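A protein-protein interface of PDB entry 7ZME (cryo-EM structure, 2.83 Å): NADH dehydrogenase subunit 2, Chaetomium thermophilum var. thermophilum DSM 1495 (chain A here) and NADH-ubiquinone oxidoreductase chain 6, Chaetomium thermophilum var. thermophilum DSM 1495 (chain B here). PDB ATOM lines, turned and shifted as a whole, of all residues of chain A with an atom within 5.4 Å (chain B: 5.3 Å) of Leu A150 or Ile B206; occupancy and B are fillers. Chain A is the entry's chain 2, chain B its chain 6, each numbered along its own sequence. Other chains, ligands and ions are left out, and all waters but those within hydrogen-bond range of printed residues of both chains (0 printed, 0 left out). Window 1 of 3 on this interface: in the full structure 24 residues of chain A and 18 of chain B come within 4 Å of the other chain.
OG of Ser A147 is in hydrogen-bond range of NE1 of Trp B199.
The side-chain carboxylate of Glu A153 is in hydrogen-bond range of the side-chain hydroxyl of Tyr A157 (2.5 Å).
The backbone carbonyl oxygen (O) of Ser A147 is in hydrogen-bond range of the side-chain hydroxyl (OG) of Ser A151 (2.9 Å).
Among the printed residues, pairs that only touch across the chains: Val A146 with Trp B199 (3.5 Å), Leu A150 with Trp B199 (3.9 Å), Leu A150 with Ile B206 (3.6 Å), Leu A154 with Phe B205 (3.7 Å), Leu A154 with Ile B206 (3.9 Å), Leu A154 with Leu B209 (3.9 Å), Tyr A157 with Ile B206 (3.6 Å) and Tyr A157 with Leu B209 (3.8 Å).
Ile B206 touches just these residues of chain A: Leu A150, Leu A154 and Tyr A157.
Printed residues of chain A within 4 Å of Trp B199: Val A146, Ser A147 and Leu A150.
Of the printed residues of chain B, Tyr A157 touches Ile B206 (3.6 Å) and Leu B209 (3.8 Å).
Hydrophobic or aromatic side chains of chain B that line the printed part of chain A: Trp B199, Ile B206 and Leu B209.
Of the 11 printed residues of chain A, 5 touch a printed residue of chain B.
Printed residues of chain A that touch a printed residue of chain B: Val A146, Ser A147, Leu A150, Leu A154 and Tyr A157.
Among the printed residues, no Asp or Glu carboxylate lies within 4 Å of a Lys or Arg side-chain nitrogen of the other chain.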
ATOM      1  N   VAL A 146     -13.519  12.700 -20.659  1.00  0.00           N
ATOM      2  CA  VAL A 146     -14.858  12.494 -21.204  1.00  0.00           C
ATOM      3  C   VAL A 146     -15.909  13.084 -20.271  1.00  0.00           C
ATOM      4  O   VAL A 146     -16.928  13.619 -20.724  1.00  0.00           O
ATOM      5  CB  VAL A 146     -15.099  10.996 -21.470  1.00  0.00           C
ATOM      6  CG1 VAL A 146     -16.440  10.771 -22.152  1.00  0.00           C
ATOM      7  CG2 VAL A 146     -13.973  10.420 -22.306  1.00  0.00           C
ATOM      8  N   SER A 147     -15.679  12.996 -18.960  1.00  0.00           N
ATOM      9  CA  SER A 147     -16.586  13.616 -17.998  1.00  0.00           C
ATOM     10  C   SER A 147     -16.632  15.128 -18.176  1.00  0.00           C
ATOM     11  O   SER A 147     -17.700  15.739 -18.058  1.00  0.00           O
ATOM     12  CB  SER A 147     -16.163  13.264 -16.572  1.00  0.00           C
ATOM     13  OG  SER A 147     -16.010  11.870 -16.404  1.00  0.00           O
ATOM     14  N   ILE A 148     -15.482  15.750 -18.441  1.00  0.00           N
ATOM     15  CA  ILE A 148     -15.432  17.202 -18.605  1.00  0.00           C
ATOM     16  C   ILE A 148     -16.303  17.634 -19.775  1.00  0.00           C
ATOM     17  O   ILE A 148     -17.081  18.589 -19.672  1.00  0.00           O
ATOM     18  CB  ILE A 148     -13.978  17.675 -18.787  1.00  0.00           C
ATOM     19  CG1 ILE A 148     -13.200  17.567 -17.480  1.00  0.00           C
ATOM     20  CG2 ILE A 148     -13.933  19.100 -19.299  1.00  0.00           C
ATOM     21  CD1 ILE A 148     -11.707  17.504 -17.676  1.00  0.00           C
ATOM     22  N   PHE A 149     -16.185  16.935 -20.904  1.00  0.00           N
ATOM     23  CA  PHE A 149     -16.925  17.328 -22.096  1.00  0.00           C
ATOM     24  C   PHE A 149     -18.428  17.222 -21.882  1.00  0.00           C
ATOM     25  O   PHE A 149     -19.177  18.136 -22.242  1.00  0.00           O
ATOM     26  CB  PHE A 149     -16.495  16.477 -23.289  1.00  0.00           C
ATOM     27  CG  PHE A 149     -17.097  16.917 -24.589  1.00  0.00           C
ATOM     28  CD1 PHE A 149     -16.865  18.192 -25.076  1.00  0.00           C
ATOM     29  CD2 PHE A 149     -17.901  16.066 -25.317  1.00  0.00           C
ATOM     30  CE1 PHE A 149     -17.422  18.603 -26.268  1.00  0.00           C
ATOM     31  CE2 PHE A 149     -18.456  16.474 -26.507  1.00  0.00           C
ATOM     32  CZ  PHE A 149     -18.219  17.744 -26.982  1.00  0.00           C
ATOM     33  N   LEU A 150     -18.891  16.120 -21.291  1.00  0.00           N
ATOM     34  CA  LEU A 150     -20.321  15.933 -21.085  1.00  0.00           C
ATOM     35  C   LEU A 150     -20.899  16.958 -20.118  1.00  0.00           C
ATOM     36  O   LEU A 150     -22.026  17.424 -20.317  1.00  0.00           O
ATOM     37  CB  LEU A 150     -20.603  14.520 -20.573  1.00  0.00           C
ATOM     38  CG  LEU A 150     -20.223  13.340 -21.466  1.00  0.00           C
ATOM     39  CD1 LEU A 150     -20.123  12.069 -20.649  1.00  0.00           C
ATOM     40  CD2 LEU A 150     -21.212  13.158 -22.599  1.00  0.00           C
ATOM     41  N   SER A 151     -20.156  17.317 -19.074  1.00  0.00           N
ATOM     42  CA  SER A 151     -20.673  18.250 -18.082  1.00  0.00           C
ATOM     43  C   SER A 151     -20.715  19.677 -18.612  1.00  0.00           C
ATOM     44  O   SER A 151     -21.662  20.416 -18.327  1.00  0.00           O
ATOM     45  CB  SER A 151     -19.835  18.177 -16.808  1.00  0.00           C
ATOM     46  OG  SER A 151     -19.742  16.845 -16.346  1.00  0.00           O
ATOM     47  N   ILE A 152     -19.703  20.086 -19.380  1.00  0.00           N
ATOM     48  CA  ILE A 152     -19.706  21.442 -19.919  1.00  0.00           C
ATOM     49  C   ILE A 152     -20.789  21.593 -20.980  1.00  0.00           C
ATOM     50  O   ILE A 152     -21.323  22.689 -21.185  1.00  0.00           O
ATOM     51  CB  ILE A 152     -18.309  21.827 -20.447  1.00  0.00           C
ATOM     52  CG1 ILE A 152     -18.204  23.345 -20.592  1.00  0.00           C
ATOM     53  CG2 ILE A 152     -18.005  21.153 -21.772  1.00  0.00           C
ATOM     54  CD1 ILE A 152     -18.366  24.094 -19.294  1.00  0.00           C
ATOM     55  N   GLU A 153     -21.145  20.501 -21.661  1.00  0.00           N
ATOM     56  CA  GLU A 153     -22.251  20.563 -22.613  1.00  0.00           C
ATOM     57  C   GLU A 153     -23.594  20.629 -21.901  1.00  0.00           C
ATOM     58  O   GLU A 153     -24.491  21.359 -22.331  1.00  0.00           O
ATOM     59  CB  GLU A 153     -22.211  19.367 -23.560  1.00  0.00           C
ATOM     60  CG  GLU A 153     -20.983  19.299 -24.446  1.00  0.00           C
ATOM     61  CD  GLU A 153     -21.012  20.316 -25.561  1.00  0.00           C
ATOM     62  OE1 GLU A 153     -20.752  21.506 -25.291  1.00  0.00           O
ATOM     63  OE2 GLU A 153     -21.300  19.928 -26.711  1.00  0.00           O
ATOM     64  N   LEU A 154     -23.756  19.868 -20.816  1.00  0.00           N
ATOM     65  CA  LEU A 154     -24.994  19.929 -20.049  1.00  0.00           C
ATOM     66  C   LEU A 154     -25.204  21.318 -19.460  1.00  0.00           C
ATOM     67  O   LEU A 154     -26.336  21.810 -19.401  1.00  0.00           O
ATOM     68  CB  LEU A 154     -24.983  18.873 -18.948  1.00  0.00           C
ATOM     69  CG  LEU A 154     -26.291  18.644 -18.186  1.00  0.00           C
ATOM     70  CD1 LEU A 154     -27.423  18.291 -19.131  1.00  0.00           C
ATOM     71  CD2 LEU A 154     -26.112  17.567 -17.143  1.00  0.00           C
ATOM     72  N   GLN A 155     -24.127  21.961 -19.012  1.00  0.00           N
ATOM     73  CA  GLN A 155     -24.215  23.350 -18.570  1.00  0.00           C
ATOM     74  C   GLN A 155     -24.537  24.282 -19.734  1.00  0.00           C
ATOM     75  O   GLN A 155     -25.394  25.163 -19.618  1.00  0.00           O
ATOM     76  CB  GLN A 155     -22.907  23.761 -17.895  1.00  0.00           C
ATOM     77  CG  GLN A 155     -22.998  25.026 -17.062  1.00  0.00           C
ATOM     78  CD  GLN A 155     -21.651  25.685 -16.863  1.00  0.00           C
ATOM     79  OE1 GLN A 155     -20.963  25.429 -15.879  1.00  0.00           O
ATOM     80  NE2 GLN A 155     -21.263  26.533 -17.803  1.00  0.00           N
ATOM     81  N   TYR A 157     -25.807  23.717 -22.910  1.00  0.00           N
ATOM     82  CA  TYR A 157     -27.061  23.533 -23.633  1.00  0.00           C
ATOM     83  C   TYR A 157     -28.236  24.134 -22.872  1.00  0.00           C
ATOM     84  O   TYR A 157     -29.115  24.765 -23.469  1.00  0.00           O
ATOM     85  CB  TYR A 157     -27.298  22.048 -23.890  1.00  0.00           C
ATOM     86  CG  TYR A 157     -26.328  21.428 -24.864  1.00  0.00           C
ATOM     87  CD1 TYR A 157     -25.530  22.215 -25.679  1.00  0.00           C
ATOM     88  CD2 TYR A 157     -26.192  20.050 -24.948  1.00  0.00           C
ATOM     89  CE1 TYR A 157     -24.640  21.649 -26.558  1.00  0.00           C
ATOM     90  CE2 TYR A 157     -25.300  19.476 -25.825  1.00  0.00           C
ATOM     91  CZ  TYR A 157     -24.531  20.280 -26.626  1.00  0.00           C
ATOM     92  OH  TYR A 157     -23.639  19.707 -27.499  1.00  0.00           O
ATOM     93  N   TRP B 199     -20.782   8.017 -17.534  1.00  0.00           N
ATOM     94  CA  TRP B 199     -20.905   8.648 -18.839  1.00  0.00           C
ATOM     95  C   TRP B 199     -22.271   8.396 -19.453  1.00  0.00           C
ATOM     96  O   TRP B 199     -22.774   9.232 -20.206  1.00  0.00           O
ATOM     97  CB  TRP B 199     -19.809   8.140 -19.769  1.00  0.00           C
ATOM     98  CG  TRP B 199     -18.440   8.508 -19.332  1.00  0.00           C
ATOM     99  CD1 TRP B 199     -18.098   9.456 -18.418  1.00  0.00           C
ATOM    100  CD2 TRP B 199     -17.218   7.934 -19.795  1.00  0.00           C
ATOM    101  NE1 TRP B 199     -16.736   9.509 -18.280  1.00  0.00           N
ATOM    102  CE2 TRP B 199     -16.171   8.584 -19.116  1.00  0.00           C
ATOM    103  CE3 TRP B 199     -16.907   6.935 -20.719  1.00  0.00           C
ATOM    104  CZ2 TRP B 199     -14.837   8.265 -19.327  1.00  0.00           C
ATOM    105  CZ3 TRP B 199     -15.583   6.621 -20.927  1.00  0.00           C
ATOM    106  CH2 TRP B 199     -14.562   7.285 -20.236  1.00  0.00           C
ATOM    107  N   LEU B 202     -24.868  10.759 -17.451  1.00  0.00           N
ATOM    108  CA  LEU B 202     -24.716  12.126 -17.939  1.00  0.00           C
ATOM    109  C   LEU B 202     -25.205  12.266 -19.372  1.00  0.00           C
ATOM    110  O   LEU B 202     -25.878  13.244 -19.711  1.00  0.00           O
ATOM    111  CB  LEU B 202     -23.258  12.576 -17.819  1.00  0.00           C
ATOM    112  CG  LEU B 202     -22.740  13.125 -16.484  1.00  0.00           C
ATOM    113  CD1 LEU B 202     -23.463  14.409 -16.142  1.00  0.00           C
ATOM    114  CD2 LEU B 202     -22.900  12.134 -15.346  1.00  0.00           C
ATOM    115  N   ALA B 203     -24.879  11.299 -20.232  1.00  0.00           N
ATOM    116  CA  ALA B 203     -25.334  11.363 -21.616  1.00  0.00           C
ATOM    117  C   ALA B 203     -26.853  11.314 -21.700  1.00  0.00           C
ATOM    118  O   ALA B 203     -27.458  11.999 -22.529  1.00  0.00           O
ATOM    119  CB  ALA B 203     -24.716  10.230 -22.428  1.00  0.00           C
ATOM    120  N   SER B 204     -27.486  10.510 -20.846  1.00  0.00           N
ATOM    121  CA  SER B 204     -28.938  10.423 -20.834  1.00  0.00           C
ATOM    122  C   SER B 204     -29.593  11.696 -20.319  1.00  0.00           C
ATOM    123  O   SER B 204     -30.768  11.932 -20.615  1.00  0.00           O
ATOM    124  CB  SER B 204     -29.385   9.233 -19.988  1.00  0.00           C
ATOM    125  OG  SER B 204     -29.304   9.534 -18.611  1.00  0.00           O
ATOM    126  N   PHE B 205     -28.873  12.517 -19.558  1.00  0.00           N
ATOM    127  CA  PHE B 205     -29.420  13.787 -19.099  1.00  0.00           C
ATOM    128  C   PHE B 205     -29.228  14.898 -20.117  1.00  0.00           C
ATOM    129  O   PHE B 205     -30.042  15.825 -20.172  1.00  0.00           O
ATOM    130  CB  PHE B 205     -28.800  14.184 -17.757  1.00  0.00           C
ATOM    131  CG  PHE B 205     -29.642  13.799 -16.578  1.00  0.00           C
ATOM    132  CD1 PHE B 205     -29.599  12.514 -16.071  1.00  0.00           C
ATOM    133  CD2 PHE B 205     -30.508  14.710 -16.001  1.00  0.00           C
ATOM    134  CE1 PHE B 205     -30.386  12.153 -14.998  1.00  0.00           C
ATOM    135  CE2 PHE B 205     -31.298  14.355 -14.930  1.00  0.00           C
ATOM    136  CZ  PHE B 205     -31.237  13.074 -14.427  1.00  0.00           C
ATOM    137  N   ILE B 206     -28.221  14.785 -20.968  1.00  0.00           N
ATOM    138  CA  ILE B 206     -28.080  15.764 -22.082  1.00  0.00           C
ATOM    139  C   ILE B 206     -29.248  15.485 -23.032  1.00  0.00           C
ATOM    140  O   ILE B 206     -29.925  16.450 -23.418  1.00  0.00           O
ATOM    141  CB  ILE B 206     -26.701  15.625 -22.757  1.00  0.00           C
ATOM    142  CG1 ILE B 206     -25.571  15.817 -21.744  1.00  0.00           C
ATOM    143  CG2 ILE B 206     -26.568  16.572 -23.935  1.00  0.00           C
ATOM    144  CD1 ILE B 206     -24.216  15.383 -22.243  1.00  0.00           C
ATOM    145  N   LEU B 207     -29.478  14.222 -23.377  1.00  0.00           N
ATOM    146  CA  LEU B 207     -30.583  13.831 -24.286  1.00  0.00           C
ATOM    147  C   LEU B 207     -31.944  14.246 -23.720  1.00  0.00           C
ATOM    148  O   LEU B 207     -32.764  14.702 -24.513  1.00  0.00           O
ATOM    149  CB  LEU B 207     -30.539  12.310 -24.396  1.00  0.00           C
ATOM    150  CG  LEU B 207     -29.406  11.717 -25.220  1.00  0.00           C
ATOM    151  CD1 LEU B 207     -29.120  10.310 -24.739  1.00  0.00           C
ATOM    152  CD2 LEU B 207     -29.751  11.730 -26.702  1.00  0.00           C
ATOM    153  N   LEU B 208     -32.173  14.084 -22.417  1.00  0.00           N
ATOM    154  CA  LEU B 208     -33.438  14.491 -21.759  1.00  0.00           C
ATOM    155  C   LEU B 208     -33.647  16.000 -21.874  1.00  0.00           C
ATOM    156  O   LEU B 208     -34.765  16.415 -22.201  1.00  0.00           O
ATOM    157  CB  LEU B 208     -33.319  14.121 -20.279  1.00  0.00           C
ATOM    158  CG  LEU B 208     -34.604  14.165 -19.462  1.00  0.00           C
ATOM    159  CD1 LEU B 208     -35.558  13.087 -19.931  1.00  0.00           C
ATOM    160  CD2 LEU B 208     -34.291  13.985 -17.987  1.00  0.00           C
ATOM    161  N   LEU B 209     -32.610  16.784 -21.602  1.00  0.00           N
ATOM    162  CA  LEU B 209     -32.714  18.255 -21.689  1.00  0.00           C
ATOM    163  C   LEU B 209     -32.996  18.623 -23.146  1.00  0.00           C
ATOM    164  O   LEU B 209     -33.804  19.524 -23.375  1.00  0.00           O
ATOM    165  CB  LEU B 209     -31.406  18.864 -21.178  1.00  0.00           C
ATOM    166  CG  LEU B 209     -31.168  20.341 -21.476  1.00  0.00           C
ATOM    167  CD1 LEU B 209     -32.066  21.221 -20.623  1.00  0.00           C
ATOM    168  CD2 LEU B 209     -29.711  20.692 -21.245  1.00  0.00           C
ATOM    169  N   ALA B 210     -32.370  17.931 -24.095  1.00  0.00           N
ATOM    170  CA  ALA B 210     -32.629  18.199 -25.525  1.00  0.00           C
ATOM    171  C   ALA B 210     -34.069  17.838 -25.897  1.00  0.00           C
ATOM    172  O   ALA B 210     -34.692  18.601 -26.638  1.00  0.00           O
ATOM    173  CB  ALA B 210     -31.631  17.475 -26.372  1.00  0.00           C
ATOM    174  N   MET B 211     -34.576  16.719 -25.394  1.00  0.00           N
ATOM    175  CA  MET B 211     -35.968  16.286 -25.682  1.00  0.00           C
ATOM    176  C   MET B 211     -36.962  17.292 -25.104  1.00  0.00           C
ATOM    177  O   MET B 211     -37.956  17.580 -25.777  1.00  0.00           O
ATOM    178  CB  MET B 211     -36.241  14.906 -25.080  1.00  0.00           C
ATOM    179  CG  MET B 211     -35.334  13.813 -25.586  1.00  0.00           C
ATOM    180  SD  MET B 211     -35.838  12.214 -24.908  1.00  0.00           S
ATOM    181  CE  MET B 211     -37.507  12.107 -25.549  1.00  0.00           C
